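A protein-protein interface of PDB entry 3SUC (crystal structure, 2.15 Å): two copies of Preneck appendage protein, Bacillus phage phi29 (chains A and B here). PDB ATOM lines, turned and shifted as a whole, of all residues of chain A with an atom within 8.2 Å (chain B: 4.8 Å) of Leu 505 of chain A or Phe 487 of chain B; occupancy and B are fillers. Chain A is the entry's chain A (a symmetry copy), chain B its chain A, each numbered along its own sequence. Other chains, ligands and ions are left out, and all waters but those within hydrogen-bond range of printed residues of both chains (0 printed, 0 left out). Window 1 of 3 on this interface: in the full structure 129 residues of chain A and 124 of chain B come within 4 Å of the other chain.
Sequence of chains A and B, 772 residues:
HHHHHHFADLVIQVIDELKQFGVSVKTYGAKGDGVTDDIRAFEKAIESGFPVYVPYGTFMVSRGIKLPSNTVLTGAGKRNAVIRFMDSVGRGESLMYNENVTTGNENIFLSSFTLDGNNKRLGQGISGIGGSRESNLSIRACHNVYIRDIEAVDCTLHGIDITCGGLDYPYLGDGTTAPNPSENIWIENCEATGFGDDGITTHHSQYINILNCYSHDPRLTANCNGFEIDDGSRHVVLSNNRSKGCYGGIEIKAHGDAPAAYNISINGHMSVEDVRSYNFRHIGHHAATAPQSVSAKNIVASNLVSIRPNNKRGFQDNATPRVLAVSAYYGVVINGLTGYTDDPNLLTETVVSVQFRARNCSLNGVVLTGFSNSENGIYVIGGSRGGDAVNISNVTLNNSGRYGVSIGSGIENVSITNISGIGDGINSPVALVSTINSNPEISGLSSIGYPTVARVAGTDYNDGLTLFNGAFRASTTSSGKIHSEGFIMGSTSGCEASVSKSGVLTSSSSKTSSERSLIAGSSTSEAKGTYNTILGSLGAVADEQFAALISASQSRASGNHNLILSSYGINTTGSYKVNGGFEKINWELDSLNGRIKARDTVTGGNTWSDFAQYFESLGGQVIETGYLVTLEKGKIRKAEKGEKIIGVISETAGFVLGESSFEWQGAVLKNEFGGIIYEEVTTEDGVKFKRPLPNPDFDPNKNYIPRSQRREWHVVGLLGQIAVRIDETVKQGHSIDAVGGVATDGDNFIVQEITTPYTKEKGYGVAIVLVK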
ATOM      1  N   ALA A 474      -6.212 -10.396  25.908  1.00  0.00           N
ATOM      2  CA  ALA A 474      -5.508 -11.527  25.315  1.00  0.00           C
ATOM      3  C   ALA A 474      -4.877 -11.168  23.979  1.00  0.00           C
ATOM      4  O   ALA A 474      -5.453 -10.427  23.186  1.00  0.00           O
ATOM      5  CB  ALA A 474      -6.449 -12.743  25.169  1.00  0.00           C
ATOM      6  N   SER A 475      -3.680 -11.703  23.748  1.00  0.00           N
ATOM      7  CA  SER A 475      -2.948 -11.582  22.469  1.00  0.00           C
ATOM      8  C   SER A 475      -2.735 -10.149  21.964  1.00  0.00           C
ATOM      9  O   SER A 475      -2.851  -9.879  20.777  1.00  0.00           O
ATOM     10  CB  SER A 475      -3.565 -12.492  21.381  1.00  0.00           C
ATOM     11  OG  SER A 475      -4.900 -12.136  21.048  1.00  0.00           O
ATOM     12  N   THR A 476      -2.447  -9.230  22.878  1.00  0.00           N
ATOM     13  CA  THR A 476      -2.206  -7.834  22.496  1.00  0.00           C
ATOM     14  C   THR A 476      -0.849  -7.359  22.997  1.00  0.00           C
ATOM     15  O   THR A 476      -0.329  -7.848  24.005  1.00  0.00           O
ATOM     16  CB  THR A 476      -3.367  -6.851  22.920  1.00  0.00           C
ATOM     17  OG1 THR A 476      -2.966  -6.023  24.025  1.00  0.00           O
ATOM     18  CG2 THR A 476      -4.640  -7.589  23.246  1.00  0.00           C
ATOM     19  N   PHE A 487     -12.938  -5.497  27.234  1.00  0.00           N
ATOM     20  CA  PHE A 487     -11.815  -6.361  26.841  1.00  0.00           C
ATOM     21  C   PHE A 487     -11.006  -5.768  25.680  1.00  0.00           C
ATOM     22  O   PHE A 487     -11.492  -4.918  24.959  1.00  0.00           O
ATOM     23  CB  PHE A 487     -12.312  -7.766  26.468  1.00  0.00           C
ATOM     24  CG  PHE A 487     -13.301  -7.770  25.341  1.00  0.00           C
ATOM     25  CD1 PHE A 487     -14.665  -7.926  25.598  1.00  0.00           C
ATOM     26  CD2 PHE A 487     -12.875  -7.591  24.023  1.00  0.00           C
ATOM     27  CE1 PHE A 487     -15.587  -7.909  24.563  1.00  0.00           C
ATOM     28  CE2 PHE A 487     -13.776  -7.571  22.991  1.00  0.00           C
ATOM     29  CZ  PHE A 487     -15.146  -7.733  23.259  1.00  0.00           C
ATOM     30  N   ILE A 488      -9.775  -6.236  25.510  1.00  0.00           N
ATOM     31  CA  ILE A 488      -8.975  -5.918  24.323  1.00  0.00           C
ATOM     32  C   ILE A 488      -8.335  -7.212  23.822  1.00  0.00           C
ATOM     33  O   ILE A 488      -7.671  -7.898  24.580  1.00  0.00           O
ATOM     34  CB  ILE A 488      -7.894  -4.812  24.620  1.00  0.00           C
ATOM     35  CG1 ILE A 488      -8.496  -3.412  24.496  1.00  0.00           C
ATOM     36  CG2 ILE A 488      -6.757  -4.861  23.637  1.00  0.00           C
ATOM     37  CD1 ILE A 488      -8.784  -2.783  25.775  1.00  0.00           C
ATOM     38  N   MET A 489      -8.563  -7.556  22.558  1.00  0.00           N
ATOM     39  CA  MET A 489      -8.001  -8.793  21.987  1.00  0.00           C
ATOM     40  C   MET A 489      -7.383  -8.578  20.607  1.00  0.00           C
ATOM     41  O   MET A 489      -7.944  -7.865  19.772  1.00  0.00           O
ATOM     42  CB  MET A 489      -9.065  -9.901  21.901  1.00  0.00           C
ATOM     43  CG  MET A 489      -9.615 -10.417  23.238  1.00  0.00           C
ATOM     44  SD  MET A 489     -10.607 -11.927  22.993  1.00  0.00           S
ATOM     45  CE  MET A 489      -9.314 -13.130  22.778  1.00  0.00           C
ATOM     46  N   GLY A 490      -6.226  -9.207  20.385  1.00  0.00           N
ATOM     47  CA  GLY A 490      -5.539  -9.215  19.073  1.00  0.00           C
ATOM     48  C   GLY A 490      -5.227  -7.818  18.583  1.00  0.00           C
ATOM     49  O   GLY A 490      -5.400  -7.500  17.414  1.00  0.00           O
ATOM     50  N   SER A 491      -4.783  -6.977  19.505  1.00  0.00           N
ATOM     51  CA  SER A 491      -4.778  -5.536  19.291  1.00  0.00           C
ATOM     52  C   SER A 491      -3.423  -4.935  19.617  1.00  0.00           C
ATOM     53  O   SER A 491      -2.644  -5.524  20.354  1.00  0.00           O
ATOM     54  CB  SER A 491      -5.888  -4.894  20.136  1.00  0.00           C
ATOM     55  OG  SER A 491      -7.122  -4.910  19.440  1.00  0.00           O
ATOM     56  N   THR A 492      -3.130  -3.765  19.063  1.00  0.00           N
ATOM     57  CA  THR A 492      -1.807  -3.158  19.297  1.00  0.00           C
ATOM     58  C   THR A 492      -1.857  -1.665  19.609  1.00  0.00           C
ATOM     59  O   THR A 492      -2.809  -0.974  19.263  1.00  0.00           O
ATOM     60  CB  THR A 492      -0.832  -3.386  18.104  1.00  0.00           C
ATOM     61  OG1 THR A 492      -1.275  -2.631  16.975  1.00  0.00           O
ATOM     62  CG2 THR A 492      -0.741  -4.860  17.725  1.00  0.00           C
ATOM     63  N   CYS A 495      -4.646   0.385  22.675  1.00  0.00           N
ATOM     64  CA  CYS A 495      -6.079   0.169  22.552  1.00  0.00           C
ATOM     65  C   CYS A 495      -6.726   0.204  23.927  1.00  0.00           C
ATOM     66  O   CYS A 495      -6.219  -0.376  24.880  1.00  0.00           O
ATOM     67  CB  CYS A 495      -6.373  -1.152  21.839  1.00  0.00           C
ATOM     68  SG  CYS A 495      -6.386  -0.984  20.063  1.00  0.00           S
ATOM     69  N   ALA A 497     -10.521   0.325  26.275  1.00  0.00           N
ATOM     70  CA  ALA A 497     -11.970   0.075  26.380  1.00  0.00           C
ATOM     71  C   ALA A 497     -12.414   0.464  27.783  1.00  0.00           C
ATOM     72  O   ALA A 497     -12.420  -0.362  28.695  1.00  0.00           O
ATOM     73  CB  ALA A 497     -12.294  -1.399  26.088  1.00  0.00           C
ATOM     74  N   SER A 502     -17.738  -2.399  26.650  1.00  0.00           N
ATOM     75  CA  SER A 502     -16.960  -1.810  25.557  1.00  0.00           C
ATOM     76  C   SER A 502     -15.849  -2.784  25.210  1.00  0.00           C
ATOM     77  O   SER A 502     -15.319  -3.440  26.086  1.00  0.00           O
ATOM     78  CB  SER A 502     -16.384  -0.440  25.955  1.00  0.00           C
ATOM     79  OG  SER A 502     -15.494  -0.559  27.057  1.00  0.00           O
ATOM     80  N   GLY A 503     -15.510  -2.908  23.934  1.00  0.00           N
ATOM     81  CA  GLY A 503     -14.522  -3.916  23.524  1.00  0.00           C
ATOM     82  C   GLY A 503     -13.751  -3.543  22.283  1.00  0.00           C
ATOM     83  O   GLY A 503     -14.277  -2.876  21.408  1.00  0.00           O
ATOM     84  N   VAL A 504     -12.487  -3.957  22.210  1.00  0.00           N
ATOM     85  CA  VAL A 504     -11.685  -3.690  21.006  1.00  0.00           C
ATOM     86  C   VAL A 504     -11.033  -4.959  20.470  1.00  0.00           C
ATOM     87  O   VAL A 504     -10.369  -5.677  21.198  1.00  0.00           O
ATOM     88  CB  VAL A 504     -10.611  -2.578  21.240  1.00  0.00           C
ATOM     89  CG1 VAL A 504      -9.829  -2.324  19.963  1.00  0.00           C
ATOM     90  CG2 VAL A 504     -11.272  -1.278  21.723  1.00  0.00           C
ATOM     91  N   LEU A 505     -11.233  -5.223  19.185  1.00  0.00           N
ATOM     92  CA  LEU A 505     -10.614  -6.385  18.547  1.00  0.00           C
ATOM     93  C   LEU A 505      -9.718  -5.988  17.380  1.00  0.00           C
ATOM     94  O   LEU A 505     -10.027  -5.053  16.640  1.00  0.00           O
ATOM     95  CB  LEU A 505     -11.691  -7.358  18.033  1.00  0.00           C
ATOM     96  CG  LEU A 505     -12.716  -7.935  19.011  1.00  0.00           C
ATOM     97  CD1 LEU A 505     -13.785  -8.728  18.245  1.00  0.00           C
ATOM     98  CD2 LEU A 505     -12.034  -8.797  20.036  1.00  0.00           C
ATOM     99  N   THR A 506      -8.614  -6.716  17.230  1.00  0.00           N
ATOM    100  CA  THR A 506      -7.760  -6.698  16.012  1.00  0.00           C
ATOM    101  C   THR A 506      -7.515  -5.292  15.431  1.00  0.00           C
ATOM    102  O   THR A 506      -7.699  -5.031  14.244  1.00  0.00           O
ATOM    103  CB  THR A 506      -8.333  -7.655  14.950  1.00  0.00           C
ATOM    104  OG1 THR A 506      -9.698  -7.323  14.707  1.00  0.00           O
ATOM    105  CG2 THR A 506      -8.268  -9.082  15.437  1.00  0.00           C
ATOM    106  N   SER A 507      -7.112  -4.385  16.305  1.00  0.00           N
ATOM    107  CA  SER A 507      -7.120  -2.953  16.032  1.00  0.00           C
ATOM    108  C   SER A 507      -5.839  -2.346  16.561  1.00  0.00           C
ATOM    109  O   SER A 507      -5.201  -2.918  17.445  1.00  0.00           O
ATOM    110  CB  SER A 507      -8.303  -2.293  16.752  1.00  0.00           C
ATOM    111  OG  SER A 507      -9.464  -2.262  15.949  1.00  0.00           O
ATOM    112  N   SER A 508      -5.474  -1.178  16.036  1.00  0.00           N
ATOM    113  CA  SER A 508      -4.325  -0.441  16.562  1.00  0.00           C
ATOM    114  C   SER A 508      -4.726   0.964  16.994  1.00  0.00           C
ATOM    115  O   SER A 508      -5.457   1.640  16.295  1.00  0.00           O
ATOM    116  CB  SER A 508      -3.185  -0.395  15.539  1.00  0.00           C
ATOM    117  OG  SER A 508      -3.601   0.244  14.343  1.00  0.00           O
ATOM    118  N   SER A 510      -6.821   2.404  19.127  1.00  0.00           N
ATOM    119  CA  SER A 510      -8.251   2.664  19.015  1.00  0.00           C
ATOM    120  C   SER A 510      -8.843   2.777  20.405  1.00  0.00           C
ATOM    121  O   SER A 510      -8.402   2.102  21.314  1.00  0.00           O
ATOM    122  CB  SER A 510      -8.932   1.528  18.250  1.00  0.00           C
ATOM    123  OG  SER A 510      -8.671   1.632  16.871  1.00  0.00           O
ATOM    124  N   THR A 512     -12.481   3.013  22.855  1.00  0.00           N
ATOM    125  CA  THR A 512     -13.916   3.129  23.075  1.00  0.00           C
ATOM    126  C   THR A 512     -14.224   3.546  24.501  1.00  0.00           C
ATOM    127  O   THR A 512     -13.668   2.998  25.453  1.00  0.00           O
ATOM    128  CB  THR A 512     -14.725   1.865  22.659  1.00  0.00           C
ATOM    129  OG1 THR A 512     -16.075   2.006  23.120  1.00  0.00           O
ATOM    130  CG2 THR A 512     -14.118   0.591  23.230  1.00  0.00           C
ATOM    131  N   SER A 517     -20.555  -1.301  22.916  1.00  0.00           N
ATOM    132  CA  SER A 517     -19.850  -0.956  21.674  1.00  0.00           C
ATOM    133  C   SER A 517     -18.843  -2.016  21.250  1.00  0.00           C
ATOM    134  O   SER A 517     -18.400  -2.824  22.056  1.00  0.00           O
ATOM    135  CB  SER A 517     -19.142   0.397  21.817  1.00  0.00           C
ATOM    136  OG  SER A 517     -18.195   0.344  22.862  1.00  0.00           O
ATOM    137  N   LEU A 518     -18.490  -1.998  19.972  1.00  0.00           N
ATOM    138  CA  LEU A 518     -17.391  -2.821  19.468  1.00  0.00           C
ATOM    139  C   LEU A 518     -16.560  -2.066  18.439  1.00  0.00           C
ATOM    140  O   LEU A 518     -17.103  -1.417  17.555  1.00  0.00           O
ATOM    141  CB  LEU A 518     -17.919  -4.130  18.855  1.00  0.00           C
ATOM    142  CG  LEU A 518     -16.859  -5.093  18.315  1.00  0.00           C
ATOM    143  CD1 LEU A 518     -16.047  -5.719  19.462  1.00  0.00           C
ATOM    144  CD2 LEU A 518     -17.480  -6.160  17.446  1.00  0.00           C
ATOM    145  N   ILE A 519     -15.241  -2.153  18.571  1.00  0.00           N
ATOM    146  CA  ILE A 519     -14.325  -1.738  17.503  1.00  0.00           C
ATOM    147  C   ILE A 519     -13.530  -2.962  17.039  1.00  0.00           C
ATOM    148  O   ILE A 519     -12.951  -3.669  17.851  1.00  0.00           O
ATOM    149  CB  ILE A 519     -13.347  -0.621  17.964  1.00  0.00           C
ATOM    150  CG1 ILE A 519     -14.105   0.679  18.268  1.00  0.00           C
ATOM    151  CG2 ILE A 519     -12.246  -0.377  16.912  1.00  0.00           C
ATOM    152  CD1 ILE A 519     -13.248   1.754  18.958  1.00  0.00           C
ATOM    153  N   ALA A 520     -13.507  -3.210  15.735  1.00  0.00           N
ATOM    154  CA  ALA A 520     -12.763  -4.349  15.199  1.00  0.00           C
ATOM    155  C   ALA A 520     -12.104  -4.022  13.871  1.00  0.00           C
ATOM    156  O   ALA A 520     -12.608  -3.181  13.123  1.00  0.00           O
ATOM    157  CB  ALA A 520     -13.685  -5.589  15.058  1.00  0.00           C
ATOM    158  N   GLY A 521     -10.982  -4.697  13.592  1.00  0.00           N
ATOM    159  CA  GLY A 521     -10.247  -4.576  12.320  1.00  0.00           C
ATOM    160  C   GLY A 521      -9.916  -3.145  11.943  1.00  0.00           C
ATOM    161  O   GLY A 521     -10.120  -2.723  10.820  1.00  0.00           O
ATOM    162  N   SER A 522      -9.404  -2.385  12.892  1.00  0.00           N
ATOM    163  CA  SER A 522      -9.384  -0.948  12.722  1.00  0.00           C
ATOM    164  C   SER A 522      -8.067  -0.289  13.124  1.00  0.00           C
ATOM    165  O   SER A 522      -7.180  -0.922  13.700  1.00  0.00           O
ATOM    166  CB  SER A 522     -10.555  -0.328  13.497  1.00  0.00           C
ATOM    167  OG  SER A 522     -11.754  -0.404  12.747  1.00  0.00           O
ATOM    168  N   SER A 523      -7.955   0.990  12.793  1.00  0.00           N
ATOM    169  CA  SER A 523      -6.884   1.820  13.330  1.00  0.00           C
ATOM    170  C   SER A 523      -7.337   3.249  13.522  1.00  0.00           C
ATOM    171  O   SER A 523      -8.382   3.675  13.062  1.00  0.00           O
ATOM    172  CB  SER A 523      -5.630   1.770  12.444  1.00  0.00           C
ATOM    173  OG  SER A 523      -5.852   2.435  11.221  1.00  0.00           O
ATOM    174  N   ILE A 534     -17.621   0.035  15.079  1.00  0.00           N
ATOM    175  CA  ILE A 534     -16.700   0.515  14.048  1.00  0.00           C
ATOM    176  C   ILE A 534     -15.948  -0.679  13.468  1.00  0.00           C
ATOM    177  O   ILE A 534     -15.288  -1.399  14.198  1.00  0.00           O
ATOM    178  CB  ILE A 534     -15.707   1.579  14.614  1.00  0.00           C
ATOM    179  CG1 ILE A 534     -16.464   2.855  15.018  1.00  0.00           C
ATOM    180  CG2 ILE A 534     -14.610   1.900  13.605  1.00  0.00           C
ATOM    181  CD1 ILE A 534     -15.698   3.759  15.986  1.00  0.00           C
ATOM    182  N   LEU A 535     -16.057  -0.882  12.159  1.00  0.00           N
ATOM    183  CA  LEU A 535     -15.453  -2.060  11.510  1.00  0.00           C
ATOM    184  C   LEU A 535     -14.619  -1.702  10.291  1.00  0.00           C
ATOM    185  O   LEU A 535     -15.048  -0.914   9.446  1.00  0.00           O
ATOM    186  CB  LEU A 535     -16.532  -3.062  11.078  1.00  0.00           C
ATOM    187  CG  LEU A 535     -17.425  -3.735  12.123  1.00  0.00           C
ATOM    188  CD1 LEU A 535     -18.468  -4.589  11.402  1.00  0.00           C
ATOM    189  CD2 LEU A 535     -16.609  -4.565  13.095  1.00  0.00           C
ATOM    190  N   GLY A 536     -13.430  -2.300  10.214  1.00  0.00           N
ATOM    191  CA  GLY A 536     -12.530  -2.152   9.056  1.00  0.00           C
ATOM    192  C   GLY A 536     -12.310  -0.705   8.694  1.00  0.00           C
ATOM    193  O   GLY A 536     -12.479  -0.310   7.553  1.00  0.00           O
ATOM    194  N   PHE B 472      -3.942 -16.697  21.022  1.00  0.00           N
ATOM    195  CA  PHE B 472      -5.059 -17.036  21.903  1.00  0.00           C
ATOM    196  C   PHE B 472      -6.139 -17.886  21.240  1.00  0.00           C
ATOM    197  O   PHE B 472      -6.533 -17.650  20.095  1.00  0.00           O
ATOM    198  CB  PHE B 472      -5.687 -15.777  22.515  1.00  0.00           C
ATOM    199  CG  PHE B 472      -6.667 -16.066  23.619  1.00  0.00           C
ATOM    200  CD1 PHE B 472      -6.219 -16.364  24.901  1.00  0.00           C
ATOM    201  CD2 PHE B 472      -8.040 -16.062  23.374  1.00  0.00           C
ATOM    202  CE1 PHE B 472      -7.134 -16.637  25.931  1.00  0.00           C
ATOM    203  CE2 PHE B 472      -8.955 -16.332  24.397  1.00  0.00           C
ATOM    204  CZ  PHE B 472      -8.506 -16.623  25.671  1.00  0.00           C
ATOM    205  N   ILE B 482      -2.222 -19.490  14.464  1.00  0.00           N
ATOM    206  CA  ILE B 482      -2.633 -18.304  15.207  1.00  0.00           C
ATOM    207  C   ILE B 482      -1.414 -17.439  15.529  1.00  0.00           C
ATOM    208  O   ILE B 482      -0.535 -17.844  16.277  1.00  0.00           O
ATOM    209  CB  ILE B 482      -3.433 -18.650  16.502  1.00  0.00           C
ATOM    210  CG1 ILE B 482      -4.585 -19.622  16.187  1.00  0.00           C
ATOM    211  CG2 ILE B 482      -3.959 -17.370  17.161  1.00  0.00           C
ATOM    212  CD1 ILE B 482      -5.210 -20.295  17.400  1.00  0.00           C
ATOM    213  N   GLU B 485      -0.599 -11.902  17.823  1.00  0.00           N
ATOM    214  CA  GLU B 485      -1.612 -10.852  17.887  1.00  0.00           C
ATOM    215  C   GLU B 485      -2.874 -11.261  17.125  1.00  0.00           C
ATOM    216  O   GLU B 485      -3.546 -10.428  16.521  1.00  0.00           O
ATOM    217  CB  GLU B 485      -1.064  -9.512  17.373  1.00  0.00           C
ATOM    218  CG  GLU B 485       0.068  -8.911  18.217  1.00  0.00           C
ATOM    219  CD  GLU B 485       1.404  -8.861  17.486  1.00  0.00           C
ATOM    220  OE1 GLU B 485       1.506  -8.141  16.464  1.00  0.00           O
ATOM    221  OE2 GLU B 485       2.357  -9.521  17.945  1.00  0.00           O
ATOM    222  N   GLY B 486      -3.174 -12.555  17.150  1.00  0.00           N
ATOM    223  CA  GLY B 486      -4.384 -13.110  16.531  1.00  0.00           C
ATOM    224  C   GLY B 486      -5.103 -13.952  17.565  1.00  0.00           C
ATOM    225  O   GLY B 486      -4.511 -14.327  18.572  1.00  0.00           O
ATOM    226  N   PHE B 487      -6.382 -14.233  17.322  1.00  0.00           N
ATOM    227  CA  PHE B 487      -7.152 -15.147  18.181  1.00  0.00           C
ATOM    228  C   PHE B 487      -8.181 -15.960  17.386  1.00  0.00           C
ATOM    229  O   PHE B 487      -8.554 -15.584  16.291  1.00  0.00           O
ATOM    230  CB  PHE B 487      -7.853 -14.375  19.309  1.00  0.00           C
ATOM    231  CG  PHE B 487      -8.795 -13.319  18.814  1.00  0.00           C
ATOM    232  CD1 PHE B 487      -8.424 -11.972  18.835  1.00  0.00           C
ATOM    233  CD2 PHE B 487     -10.046 -13.670  18.301  1.00  0.00           C
ATOM    234  CE1 PHE B 487      -9.282 -10.994  18.359  1.00  0.00           C
ATOM    235  CE2 PHE B 487     -10.904 -12.712  17.826  1.00  0.00           C
ATOM    236  CZ  PHE B 487     -10.521 -11.360  17.855  1.00  0.00           C
ATOM    237  N   ILE B 488      -8.637 -17.069  17.959  1.00  0.00           N
ATOM    238  CA  ILE B 488      -9.771 -17.821  17.412  1.00  0.00           C
ATOM    239  C   ILE B 488     -10.706 -18.175  18.567  1.00  0.00           C
ATOM    240  O   ILE B 488     -10.273 -18.757  19.546  1.00  0.00           O
ATOM    241  CB  ILE B 488      -9.303 -19.105  16.629  1.00  0.00           C
ATOM    242  CG1 ILE B 488      -8.935 -18.760  15.186  1.00  0.00           C
ATOM    243  CG2 ILE B 488     -10.395 -20.136  16.542  1.00  0.00           C
ATOM    244  CD1 ILE B 488      -7.501 -18.691  14.949  1.00  0.00           C
ATOM    245  N   MET B 489     -11.975 -17.792  18.464  1.00  0.00           N
ATOM    246  CA  MET B 489     -12.951 -18.073  19.532  1.00  0.00           C
ATOM    247  C   MET B 489     -14.275 -18.614  18.996  1.00  0.00           C
ATOM    248  O   MET B 489     -14.785 -18.131  17.982  1.00  0.00           O
ATOM    249  CB  MET B 489     -13.221 -16.822  20.385  1.00  0.00           C
ATOM    250  CG  MET B 489     -12.035 -16.290  21.201  1.00  0.00           C
ATOM    251  SD  MET B 489     -12.581 -15.024  22.393  1.00  0.00           S
ATOM    252  CE  MET B 489     -13.303 -16.055  23.650  1.00  0.00           C
ATOM    253  N   ALA B 497      -5.897 -17.593  11.925  1.00  0.00           N
ATOM    254  CA  ALA B 497      -5.685 -16.135  11.973  1.00  0.00           C
ATOM    255  C   ALA B 497      -4.184 -15.877  11.977  1.00  0.00           C
ATOM    256  O   ALA B 497      -3.562 -15.790  13.035  1.00  0.00           O
ATOM    257  CB  ALA B 497      -6.351 -15.526  13.218  1.00  0.00           C
ATOM    258  N   SER B 502      -5.415 -10.049  13.510  1.00  0.00           N
ATOM    259  CA  SER B 502      -6.378 -10.837  12.735  1.00  0.00           C
ATOM    260  C   SER B 502      -7.134 -11.722  13.710  1.00  0.00           C
ATOM    261  O   SER B 502      -6.564 -12.187  14.677  1.00  0.00           O
ATOM    262  CB  SER B 502      -5.674 -11.681  11.660  1.00  0.00           C
ATOM    263  OG  SER B 502      -4.778 -12.615  12.248  1.00  0.00           O
ATOM    264  N   GLY B 503      -8.423 -11.934  13.480  1.00  0.00           N
ATOM    265  CA  GLY B 503      -9.233 -12.688  14.449  1.00  0.00           C
ATOM    266  C   GLY B 503     -10.399 -13.418  13.829  1.00  0.00           C
ATOM    267  O   GLY B 503     -10.965 -12.958  12.853  1.00  0.00           O
ATOM    268  N   VAL B 504     -10.750 -14.575  14.386  1.00  0.00           N
ATOM    269  CA  VAL B 504     -11.915 -15.319  13.883  1.00  0.00           C
ATOM    270  C   VAL B 504     -12.879 -15.686  15.006  1.00  0.00           C
ATOM    271  O   VAL B 504     -12.483 -16.261  16.005  1.00  0.00           O
ATOM    272  CB  VAL B 504     -11.505 -16.592  13.074  1.00  0.00           C
ATOM    273  CG1 VAL B 504     -12.741 -17.309  12.557  1.00  0.00           C
ATOM    274  CG2 VAL B 504     -10.583 -16.219  11.903  1.00  0.00           C
ATOM    275  N   LEU B 505     -14.147 -15.344  14.825  1.00  0.00           N
ATOM    276  CA  LEU B 505     -15.171 -15.691  15.811  1.00  0.00           C
ATOM    277  C   LEU B 505     -16.275 -16.553  15.210  1.00  0.00           C
ATOM    278  O   LEU B 505     -16.664 -16.364  14.057  1.00  0.00           O
ATOM    279  CB  LEU B 505     -15.805 -14.418  16.402  1.00  0.00           C
ATOM    280  CG  LEU B 505     -14.917 -13.382  17.092  1.00  0.00           C
ATOM    281  CD1 LEU B 505     -15.739 -12.132  17.439  1.00  0.00           C
ATOM    282  CD2 LEU B 505     -14.286 -13.971  18.323  1.00  0.00           C
ATOM    283  N   LEU B 518     -11.531  -8.878  10.948  1.00  0.00           N
ATOM    284  CA  LEU B 518     -12.389  -9.768  11.730  1.00  0.00           C
ATOM    285  C   LEU B 518     -13.250 -10.642  10.827  1.00  0.00           C
ATOM    286  O   LEU B 518     -13.827 -10.161   9.863  1.00  0.00           O
ATOM    287  CB  LEU B 518     -13.285  -8.965  12.688  1.00  0.00           C
ATOM    288  CG  LEU B 518     -14.214  -9.787  13.585  1.00  0.00           C
ATOM    289  CD1 LEU B 518     -13.415 -10.557  14.650  1.00  0.00           C
ATOM    290  CD2 LEU B 518     -15.271  -8.918  14.223  1.00  0.00           C
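The backbone carbonyl oxygen (O) of Gly 486 of chain B sits at hydrogen-bond distance from the side-chain hydroxyl (OG) of Ser 475 of chain A, 3.3 Å away. SD of Met 489 of chain A lies close to SD of Met 489 of chain B, 3.7 Å away.
The backbone NH of Phe 472 of chain B sits at hydrogen-bond distance from the backbone carbonyl oxygen of Gly 486 of chain B, at 3.5 Å. OG of Ser 502 of chain B lies close to O of Ala 497 of chain B. The backbone carbonyl oxygen of Ala 474 of chain A sits at hydrogen-bond distance from the backbone NH of Gly 490 of chain A (3.2 Å). N of Met 489 of chain A lies within hydrogen-bond range of O of Val 504 of chain A. O of Leu 505 of chain A is in hydrogen-bond range of N of Gly 521 of chain A (3.2 Å).
Ala 474 of chain A touches Phe 472 of chain B (CB to CD1, 3.6 Å). Glu 485 of chain B touches Ser 475 of chain A (CA to O, 3.3 Å). Met 489 of chain A touches Phe 472 of chain B (CE to CD2, 3.3 Å). Phe 487 of chain B touches Met 489 of chain A. Gly 490 of chain A touches Glu 485 of chain B (CA to O, 3.5 Å). Phe 487 of chain B touches Gly 490 of chain A (CD1 to N, 3.9 Å). Leu 505 of chain A touches Phe 487 of chain B. CE1 of Phe 487 of chain B touches CG2 of Thr 506 of chain A (3.6 Å). Gly 503 of chain B touches Thr 506 of chain A (N to CG2, 3.5 Å). Ala 520 of chain A touches Leu 518 of chain B (CB to CD2, 3.8 Å).
Of the printed residues of chain B, Ala 474 of chain A touches Phe 472. Of the printed residues of chain B, Ser 475 of chain A touches Glu 485 and Gly 486. Of the printed residues of chain B, Leu 505 of chain A touches Phe 487. Ser 510 of chain A touches none of the printed residues of chain B. Of the printed residues of chain B, Ala 520 of chain A touches Leu 518. Ser 522 of chain A touches none of the printed residues of chain B. Gly 486 of chain B touches just one residue of chain A: Ser 475. Of the printed residues of chain A, Phe 487 of chain B touches Met 489, Gly 490, Leu 505 and Thr 506. The nearest residue of chain A that does not touch Phe 487 of chain B is Ser 475 of chain A (4.1 Å). The nearest printed residue of chain A that does not touch Met 489 of chain B is Leu 505 of chain A (6.7 Å).
Hydrophobic or aromatic side chains of chain B that line the printed part of chain A: Phe 472, Phe 487, Met 489 and Leu 518. Among the printed residues, no Asp or Glu carboxylate lies within 4 Å of a Lys or Arg side-chain nitrogen of the other chain.
Met 489 of chain A touches Phe 487 of chain B, but with the chains exchanged Phe 487 of chain A does not touch Met 489 of chain B (7.6 Å). Met 489 of chain A touches its own counterpart, Met 489 of chain B. Leu 505 of chain A touches Phe 487 of chain B, but with the chains exchanged Phe 487 of chain A does not touch Leu 505 of chain B (7.3 Å). 9 positions are printed for both chains. Of the 13 pairs that touch across the chains among the printed residues, 1 has its exchanged pair printed and touching as well.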
